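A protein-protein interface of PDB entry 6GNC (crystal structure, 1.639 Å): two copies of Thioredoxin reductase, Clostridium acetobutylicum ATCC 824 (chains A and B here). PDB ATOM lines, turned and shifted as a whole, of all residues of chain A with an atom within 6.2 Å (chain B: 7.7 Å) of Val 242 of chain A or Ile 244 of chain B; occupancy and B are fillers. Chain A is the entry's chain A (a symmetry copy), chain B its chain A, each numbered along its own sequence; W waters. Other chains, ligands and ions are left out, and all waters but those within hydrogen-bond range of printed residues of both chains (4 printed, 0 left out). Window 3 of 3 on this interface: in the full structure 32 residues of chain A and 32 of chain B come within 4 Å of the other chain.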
ATOM      1  N   LEU A 234      19.288 -34.656  30.378  1.00  0.00           N
ATOM      2  CA  LEU A 234      17.889 -34.852  30.012  1.00  0.00           C
ATOM      3  C   LEU A 234      17.746 -35.345  28.574  1.00  0.00           C
ATOM      4  O   LEU A 234      18.256 -34.727  27.634  1.00  0.00           O
ATOM      5  CB  LEU A 234      17.100 -33.556  30.164  1.00  0.00           C
ATOM      6  CG  LEU A 234      16.531 -33.313  31.557  1.00  0.00           C
ATOM      7  CD1 LEU A 234      15.772 -31.993  31.545  1.00  0.00           C
ATOM      8  CD2 LEU A 234      15.658 -34.448  32.053  1.00  0.00           C
ATOM      9  N   ILE A 240      19.308 -36.800  22.991  1.00  0.00           N
ATOM     10  CA  ILE A 240      19.533 -35.716  23.946  1.00  0.00           C
ATOM     11  C   ILE A 240      18.585 -34.569  23.622  1.00  0.00           C
ATOM     12  O   ILE A 240      18.433 -34.191  22.456  1.00  0.00           O
ATOM     13  CB  ILE A 240      20.993 -35.243  23.911  1.00  0.00           C
ATOM     14  CG1 ILE A 240      21.947 -36.408  24.205  1.00  0.00           C
ATOM     15  CG2 ILE A 240      21.234 -34.086  24.895  1.00  0.00           C
ATOM     16  CD1 ILE A 240      23.376 -36.080  23.875  1.00  0.00           C
ATOM     17  N   ALA A 241      17.942 -34.004  24.645  1.00  0.00           N
ATOM     18  CA  ALA A 241      17.107 -32.819  24.425  1.00  0.00           C
ATOM     19  C   ALA A 241      18.012 -31.622  24.167  1.00  0.00           C
ATOM     20  O   ALA A 241      18.921 -31.330  24.961  1.00  0.00           O
ATOM     21  CB  ALA A 241      16.197 -32.553  25.624  1.00  0.00           C
ATOM     22  N   VAL A 242      17.799 -30.929  23.042  1.00  0.00           N
ATOM     23  CA  VAL A 242      18.608 -29.762  22.723  1.00  0.00           C
ATOM     24  C   VAL A 242      17.724 -28.610  22.285  1.00  0.00           C
ATOM     25  O   VAL A 242      16.621 -28.810  21.762  1.00  0.00           O
ATOM     26  CB  VAL A 242      19.648 -30.027  21.610  1.00  0.00           C
ATOM     27  CG1 VAL A 242      20.714 -30.986  22.087  1.00  0.00           C
ATOM     28  CG2 VAL A 242      19.001 -30.567  20.351  1.00  0.00           C
ATOM     29  N   ASP A 243      18.263 -27.402  22.418  1.00  0.00           N
ATOM     30  CA  ASP A 243      17.634 -26.233  21.808  1.00  0.00           C
ATOM     31  C   ASP A 243      18.365 -25.837  20.514  1.00  0.00           C
ATOM     32  O   ASP A 243      19.218 -26.565  19.988  1.00  0.00           O
ATOM     33  CB  ASP A 243      17.535 -25.076  22.817  1.00  0.00           C
ATOM     34  CG  ASP A 243      18.860 -24.383  23.097  1.00  0.00           C
ATOM     35  OD1 ASP A 243      19.868 -24.673  22.426  1.00  0.00           O
ATOM     36  OD2 ASP A 243      18.887 -23.523  24.006  1.00  0.00           O
ATOM     37  N   ILE A 244      17.968 -24.687  19.948  1.00  0.00           N
ATOM     38  CA  ILE A 244      18.424 -24.290  18.622  1.00  0.00           C
ATOM     39  C   ILE A 244      19.906 -24.006  18.598  1.00  0.00           C
ATOM     40  O   ILE A 244      20.521 -24.045  17.532  1.00  0.00           O
ATOM     41  CB  ILE A 244      17.623 -23.054  18.138  1.00  0.00           C
ATOM     42  CG1 ILE A 244      17.959 -22.682  16.706  1.00  0.00           C
ATOM     43  CG2 ILE A 244      17.889 -21.838  19.018  1.00  0.00           C
ATOM     44  CD1 ILE A 244      17.136 -21.504  16.286  1.00  0.00           C
ATOM     45  N   ASP A 245      20.479 -23.797  19.783  1.00  0.00           N
ATOM     46  CA  ASP A 245      21.890 -23.499  19.966  1.00  0.00           C
ATOM     47  C   ASP A 245      22.653 -24.719  20.464  1.00  0.00           C
ATOM     48  O   ASP A 245      23.823 -24.590  20.839  1.00  0.00           O
ATOM     49  CB  ASP A 245      22.036 -22.336  20.932  1.00  0.00           C
ATOM     50  CG  ASP A 245      21.481 -21.043  20.367  1.00  0.00           C
ATOM     51  OD1 ASP A 245      21.642 -20.762  19.155  1.00  0.00           O
ATOM     52  OD2 ASP A 245      20.862 -20.295  21.148  1.00  0.00           O
ATOM     53  N   MET A 246      22.005 -25.868  20.333  1.00  0.00           N
ATOM     54  CA  MET A 246      22.531 -27.149  20.776  1.00  0.00           C
ATOM     55  C   MET A 246      22.849 -27.187  22.281  1.00  0.00           C
ATOM     56  O   MET A 246      23.755 -27.905  22.686  1.00  0.00           O
ATOM     57  CB  MET A 246      23.777 -27.519  19.970  1.00  0.00           C
ATOM     58  CG  MET A 246      23.514 -27.797  18.498  1.00  0.00           C
ATOM     59  SD  MET A 246      22.285 -29.085  18.202  1.00  0.00           S
ATOM     60  CE  MET A 246      20.883 -28.110  17.670  1.00  0.00           C
ATOM     61  N   LYS A 247      22.083 -26.481  23.115  1.00  0.00           N
ATOM     62  CA  LYS A 247      22.337 -26.475  24.529  1.00  0.00           C
ATOM     63  C   LYS A 247      21.512 -27.578  25.123  1.00  0.00           C
ATOM     64  O   LYS A 247      20.411 -27.855  24.669  1.00  0.00           O
ATOM     65  CB  LYS A 247      21.880 -25.166  25.171  1.00  0.00           C
ATOM     66  CG  LYS A 247      22.674 -23.926  24.814  1.00  0.00           C
ATOM     67  CD  LYS A 247      22.275 -22.786  25.738  1.00  0.00           C
ATOM     68  CE  LYS A 247      22.473 -21.428  25.097  1.00  0.00           C
ATOM     69  NZ  LYS A 247      23.888 -21.188  24.712  1.00  0.00           N
ATOM     70  N   THR A 248      22.069 -28.231  26.123  1.00  0.00           N
ATOM     71  CA  THR A 248      21.348 -29.262  26.861  1.00  0.00           C
ATOM     72  C   THR A 248      20.889 -28.663  28.192  1.00  0.00           C
ATOM     73  O   THR A 248      21.104 -27.482  28.479  1.00  0.00           O
ATOM     74  CB  THR A 248      22.219 -30.497  27.102  1.00  0.00           C
ATOM     75  OG1 THR A 248      23.169 -30.176  28.135  1.00  0.00           O
ATOM     76  CG2 THR A 248      22.964 -30.986  25.850  1.00  0.00           C
ATOM     77  N   PHE A 254      26.930 -29.393  25.586  1.00  0.00           N
ATOM     78  CA  PHE A 254      26.254 -29.195  24.298  1.00  0.00           C
ATOM     79  C   PHE A 254      26.218 -30.524  23.571  1.00  0.00           C
ATOM     80  O   PHE A 254      26.950 -31.444  23.907  1.00  0.00           O
ATOM     81  CB  PHE A 254      26.981 -28.102  23.483  1.00  0.00           C
ATOM     82  CG  PHE A 254      27.215 -26.856  24.272  1.00  0.00           C
ATOM     83  CD1 PHE A 254      28.352 -26.722  25.059  1.00  0.00           C
ATOM     84  CD2 PHE A 254      26.253 -25.866  24.338  1.00  0.00           C
ATOM     85  CE1 PHE A 254      28.560 -25.589  25.853  1.00  0.00           C
ATOM     86  CE2 PHE A 254      26.447 -24.731  25.133  1.00  0.00           C
ATOM     87  CZ  PHE A 254      27.615 -24.591  25.884  1.00  0.00           C
ATOM     88  N   ALA A 255      25.352 -30.652  22.551  1.00  0.00           N
ATOM     89  CA  ALA A 255      25.278 -31.916  21.832  1.00  0.00           C
ATOM     90  C   ALA A 255      25.085 -31.664  20.347  1.00  0.00           C
ATOM     91  O   ALA A 255      24.651 -30.589  19.946  1.00  0.00           O
ATOM     92  CB  ALA A 255      24.156 -32.821  22.355  1.00  0.00           C
ATOM     93  N   ALA A 256      25.428 -32.672  19.552  1.00  0.00           N
ATOM     94  CA  ALA A 256      25.364 -32.513  18.085  1.00  0.00           C
ATOM     95  C   ALA A 256      25.348 -33.851  17.374  1.00  0.00           C
ATOM     96  O   ALA A 256      25.979 -34.817  17.817  1.00  0.00           O
ATOM     97  CB  ALA A 256      26.581 -31.709  17.620  1.00  0.00           C
ATOM     98  N   ALA A 260      21.557 -36.078  18.903  1.00  0.00           N
ATOM     99  CA  ALA A 260      20.686 -34.943  19.182  1.00  0.00           C
ATOM    100  C   ALA A 260      19.389 -35.013  18.388  1.00  0.00           C
ATOM    101  O   ALA A 260      18.578 -34.070  18.484  1.00  0.00           O
ATOM    102  CB  ALA A 260      21.404 -33.629  18.869  1.00  0.00           C
ATOM    103  N   GLY A 261      19.141 -36.130  17.720  1.00  0.00           N
ATOM    104  CA  GLY A 261      17.894 -36.319  17.011  1.00  0.00           C
ATOM    105  C   GLY A 261      17.943 -36.572  15.524  1.00  0.00           C
ATOM    106  O   GLY A 261      18.973 -36.440  14.876  1.00  0.00           O
ATOM    107  N   ARG A 262      16.791 -36.969  14.999  1.00  0.00           N
ATOM    108  CA  ARG A 262      16.634 -37.243  13.588  1.00  0.00           C
ATOM    109  C   ARG A 262      16.532 -35.920  12.823  1.00  0.00           C
ATOM    110  O   ARG A 262      16.180 -34.906  13.411  1.00  0.00           O
ATOM    111  CB  ARG A 262      15.399 -38.109  13.353  1.00  0.00           C
ATOM    112  CG  ARG A 262      15.600 -39.554  13.769  1.00  0.00           C
ATOM    113  CD  ARG A 262      14.431 -40.434  13.370  1.00  0.00           C
ATOM    114  NE  ARG A 262      14.614 -41.803  13.835  1.00  0.00           N
ATOM    115  CZ  ARG A 262      15.166 -42.770  13.112  1.00  0.00           C
ATOM    116  NH1 ARG A 262      15.296 -43.985  13.621  1.00  0.00           N
ATOM    117  NH2 ARG A 262      15.586 -42.525  11.879  1.00  0.00           N
ATOM    118  N   PRO A 263      16.821 -35.912  11.510  1.00  0.00           N
ATOM    119  CA  PRO A 263      17.273 -36.944  10.571  1.00  0.00           C
ATOM    120  C   PRO A 263      18.728 -37.332  10.794  1.00  0.00           C
ATOM    121  O   PRO A 263      19.516 -36.487  11.201  1.00  0.00           O
ATOM    122  CB  PRO A 263      17.118 -36.265   9.215  1.00  0.00           C
ATOM    123  CG  PRO A 263      17.336 -34.830   9.502  1.00  0.00           C
ATOM    124  CD  PRO A 263      16.743 -34.594  10.859  1.00  0.00           C
ATOM    125  N   GLN A 272      25.393 -29.111  13.155  1.00  0.00           N
ATOM    126  CA  GLN A 272      25.125 -29.059  14.591  1.00  0.00           C
ATOM    127  C   GLN A 272      26.421 -29.025  15.370  1.00  0.00           C
ATOM    128  O   GLN A 272      26.503 -28.371  16.428  1.00  0.00           O
ATOM    129  CB  GLN A 272      24.277 -30.253  15.017  1.00  0.00           C
ATOM    130  CG  GLN A 272      22.817 -30.104  14.570  1.00  0.00           C
ATOM    131  CD  GLN A 272      21.912 -31.210  15.036  1.00  0.00           C
ATOM    132  OE1 GLN A 272      22.344 -32.323  15.298  1.00  0.00           O
ATOM    133  NE2 GLN A 272      20.607 -30.918  15.079  1.00  0.00           N
ATOM    134  N   VAL B 242      12.080 -20.985  14.601  1.00  0.00           N
ATOM    135  CA  VAL B 242      12.069 -22.362  14.132  1.00  0.00           C
ATOM    136  C   VAL B 242      12.215 -23.319  15.299  1.00  0.00           C
ATOM    137  O   VAL B 242      12.797 -22.982  16.337  1.00  0.00           O
ATOM    138  CB  VAL B 242      13.187 -22.668  13.110  1.00  0.00           C
ATOM    139  CG1 VAL B 242      12.950 -21.928  11.814  1.00  0.00           C
ATOM    140  CG2 VAL B 242      14.558 -22.319  13.653  1.00  0.00           C
ATOM    141  N   ASP B 243      11.762 -24.551  15.082  1.00  0.00           N
ATOM    142  CA  ASP B 243      12.064 -25.634  16.014  1.00  0.00           C
ATOM    143  C   ASP B 243      13.195 -26.521  15.468  1.00  0.00           C
ATOM    144  O   ASP B 243      13.871 -26.197  14.482  1.00  0.00           O
ATOM    145  CB  ASP B 243      10.794 -26.428  16.359  1.00  0.00           C
ATOM    146  CG  ASP B 243      10.313 -27.344  15.244  1.00  0.00           C
ATOM    147  OD1 ASP B 243      11.013 -27.505  14.227  1.00  0.00           O
ATOM    148  OD2 ASP B 243       9.213 -27.921  15.396  1.00  0.00           O
ATOM    149  N   ILE B 244      13.454 -27.634  16.170  1.00  0.00           N
ATOM    150  CA  ILE B 244      14.621 -28.461  15.891  1.00  0.00           C
ATOM    151  C   ILE B 244      14.538 -29.114  14.532  1.00  0.00           C
ATOM    152  O   ILE B 244      15.563 -29.508  13.977  1.00  0.00           O
ATOM    153  CB  ILE B 244      14.789 -29.529  17.001  1.00  0.00           C
ATOM    154  CG1 ILE B 244      16.068 -30.328  16.836  1.00  0.00           C
ATOM    155  CG2 ILE B 244      13.619 -30.506  17.016  1.00  0.00           C
ATOM    156  CD1 ILE B 244      16.188 -31.321  17.950  1.00  0.00           C
ATOM    157  N   ASP B 245      13.325 -29.154  13.979  1.00  0.00           N
ATOM    158  CA  ASP B 245      13.039 -29.749  12.685  1.00  0.00           C
ATOM    159  C   ASP B 245      12.855 -28.682  11.614  1.00  0.00           C
ATOM    160  O   ASP B 245      12.433 -29.009  10.500  1.00  0.00           O
ATOM    161  CB  ASP B 245      11.803 -30.624  12.797  1.00  0.00           C
ATOM    162  CG  ASP B 245      12.028 -31.830  13.688  1.00  0.00           C
ATOM    163  OD1 ASP B 245      13.122 -32.442  13.659  1.00  0.00           O
ATOM    164  OD2 ASP B 245      11.094 -32.168  14.442  1.00  0.00           O
ATOM    165  N   MET B 246      13.293 -27.477  11.952  1.00  0.00           N
ATOM    166  CA  MET B 246      13.183 -26.307  11.097  1.00  0.00           C
ATOM    167  C   MET B 246      11.733 -25.970  10.712  1.00  0.00           C
ATOM    168  O   MET B 246      11.506 -25.431   9.636  1.00  0.00           O
ATOM    169  CB  MET B 246      14.029 -26.489   9.835  1.00  0.00           C
ATOM    170  CG  MET B 246      15.529 -26.538  10.085  1.00  0.00           C
ATOM    171  SD  MET B 246      16.175 -25.096  10.957  1.00  0.00           S
ATOM    172  CE  MET B 246      16.470 -25.778  12.584  1.00  0.00           C
ATOM    173  N   LYS B 247      10.763 -26.217  11.595  1.00  0.00           N
ATOM    174  CA  LYS B 247       9.390 -25.927  11.288  1.00  0.00           C
ATOM    175  C   LYS B 247       9.120 -24.535  11.776  1.00  0.00           C
ATOM    176  O   LYS B 247       9.656 -24.109  12.790  1.00  0.00           O
ATOM    177  CB  LYS B 247       8.442 -26.866  12.034  1.00  0.00           C
ATOM    178  CG  LYS B 247       8.449 -28.316  11.600  1.00  0.00           C
ATOM    179  CD  LYS B 247       7.271 -29.040  12.234  1.00  0.00           C
ATOM    180  CE  LYS B 247       7.536 -30.521  12.418  1.00  0.00           C
ATOM    181  NZ  LYS B 247       7.813 -31.207  11.131  1.00  0.00           N
ATOM    182  N   GLN B 272      20.985 -27.161   8.175  1.00  0.00           N
ATOM    183  CA  GLN B 272      19.591 -26.774   8.383  1.00  0.00           C
ATOM    184  C   GLN B 272      18.799 -26.942   7.104  1.00  0.00           C
ATOM    185  O   GLN B 272      17.607 -27.302   7.145  1.00  0.00           O
ATOM    186  CB  GLN B 272      19.507 -25.334   8.878  1.00  0.00           C
ATOM    187  CG  GLN B 272      19.934 -25.211  10.347  1.00  0.00           C
ATOM    188  CD  GLN B 272      19.791 -23.827  10.918  1.00  0.00           C
ATOM    189  OE1 GLN B 272      19.814 -22.835  10.204  1.00  0.00           O
ATOM    190  NE2 GLN B 272      19.704 -23.752  12.251  1.00  0.00           N
ATOM    191  N   ILE B 275      17.802 -30.498   7.010  1.00  0.00           N
ATOM    192  CA  ILE B 275      16.718 -30.764   7.946  1.00  0.00           C
ATOM    193  C   ILE B 275      15.399 -30.269   7.360  1.00  0.00           C
ATOM    194  O   ILE B 275      14.383 -30.966   7.403  1.00  0.00           O
ATOM    195  CB  ILE B 275      16.974 -30.089   9.296  1.00  0.00           C
ATOM    196  CG1 ILE B 275      18.234 -30.665   9.970  1.00  0.00           C
ATOM    197  CG2 ILE B 275      15.745 -30.223  10.216  1.00  0.00           C
ATOM    198  CD1 ILE B 275      18.596 -29.850  11.214  1.00  0.00           C
ATOM    199  N   ALA B 276      15.415 -29.045   6.825  1.00  0.00           N
ATOM    200  CA  ALA B 276      14.190 -28.446   6.298  1.00  0.00           C
ATOM    201  C   ALA B 276      13.647 -29.270   5.139  1.00  0.00           C
ATOM    202  O   ALA B 276      12.429 -29.496   5.044  1.00  0.00           O
ATOM    203  CB  ALA B 276      14.463 -27.015   5.832  1.00  0.00           C
ATOM    204  N   SER B 279      12.079 -32.445   6.484  1.00  0.00           N
ATOM    205  CA  SER B 279      10.794 -32.128   7.107  1.00  0.00           C
ATOM    206  C   SER B 279       9.724 -31.873   6.042  1.00  0.00           C
ATOM    207  O   SER B 279       8.575 -32.291   6.203  1.00  0.00           O
ATOM    208  CB  SER B 279      10.914 -30.926   8.035  1.00  0.00           C
ATOM    209  OG  SER B 279      11.691 -31.310   9.179  1.00  0.00           O
HETATM  210  O   HOH W   1      14.098 -34.113  15.370  1.00  0.00           O
HETATM  211  O   HOH W   2      17.008 -32.055  13.752  1.00  0.00           O
HETATM  212  O   HOH W   3      19.644 -25.486  15.005  1.00  0.00           O
HETATM  213  O   HOH W   4      18.396 -28.584  14.570  1.00  0.00           O
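Water W1 lies within hydrogen-bond range of OD1 of Asp 245 of chain B and O of Arg 262 of chain A. Water W2 bridges O of Ile 244 of chain B and O of Arg 262 of chain A. Water W4 bridges the backbone carbonyl oxygen (O) of Ile 244 of chain B (3.0 Å) and the side-chain amide nitrogen (NE2) of Gln 272 of chain A (3.3 Å). Water W3 lies within hydrogen-bond range of O of Ile 244 of chain A and NE2 of Gln 272 of chain B.
Val 242 of chain A touches Ile 244 of chain B, and with the chains exchanged Ile 244 of chain A touches Val 242 of chain B. Of the 4 pairs that touch across the chains among the printed residues, 2 have their exchanged pair printed and touching as well.
CD1 of Ile 244 of chain B touches CG2 of Val 242 of chain A, at 3.8 Å. Val 242 of chain B touches Ile 244 of chain A (CG2 to CD1, 3.8 Å). Ala 260 of chain A touches Ile 244 of chain B (O to CD1, 3.7 Å). Arg 262 of chain A touches Asp 245 of chain B.
Of the 18 printed residues of chain A, 4 touch a printed residue of chain B. Hydrophobic or aromatic side chains of chain B within 4 Å of the printed part of chain A: Val 242 and Ile 244. Among the printed residues, 4 pairs touch across the chains.
No residue of chain B comes within 4 Å of Ala 241 of chain A. Of chain B, only Ile 244 (3.8 Å) comes within 4 Å of Val 242 of chain A. Printed residues of chain B within 4 Å of Ile 244 of chain A: Val 242. Of the printed residues of chain B, Ala 260 of chain A touches Ile 244. Gly 261 of chain A touches none of the printed residues of chain B. Printed residues of chain A within 4 Å of Ile 244 of chain B: Val 242 (3.8 Å) and Ala 260 (3.7 Å). The nearest residue of chain B that does not touch Val 242 of chain A is Asp 243 of chain B (7.5 Å). The nearest residue of chain A that does not touch Ile 244 of chain B is Gln 272 of chain A (4.9 Å).
OD1 of Asp 243 of chain B lies within hydrogen-bond range of N of Asp 245 of chain B. The backbone carbonyl oxygen (O) of Asp 245 of chain B lies within hydrogen-bond range of the side-chain hydroxyl (OG) of Ser 279 of chain B.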
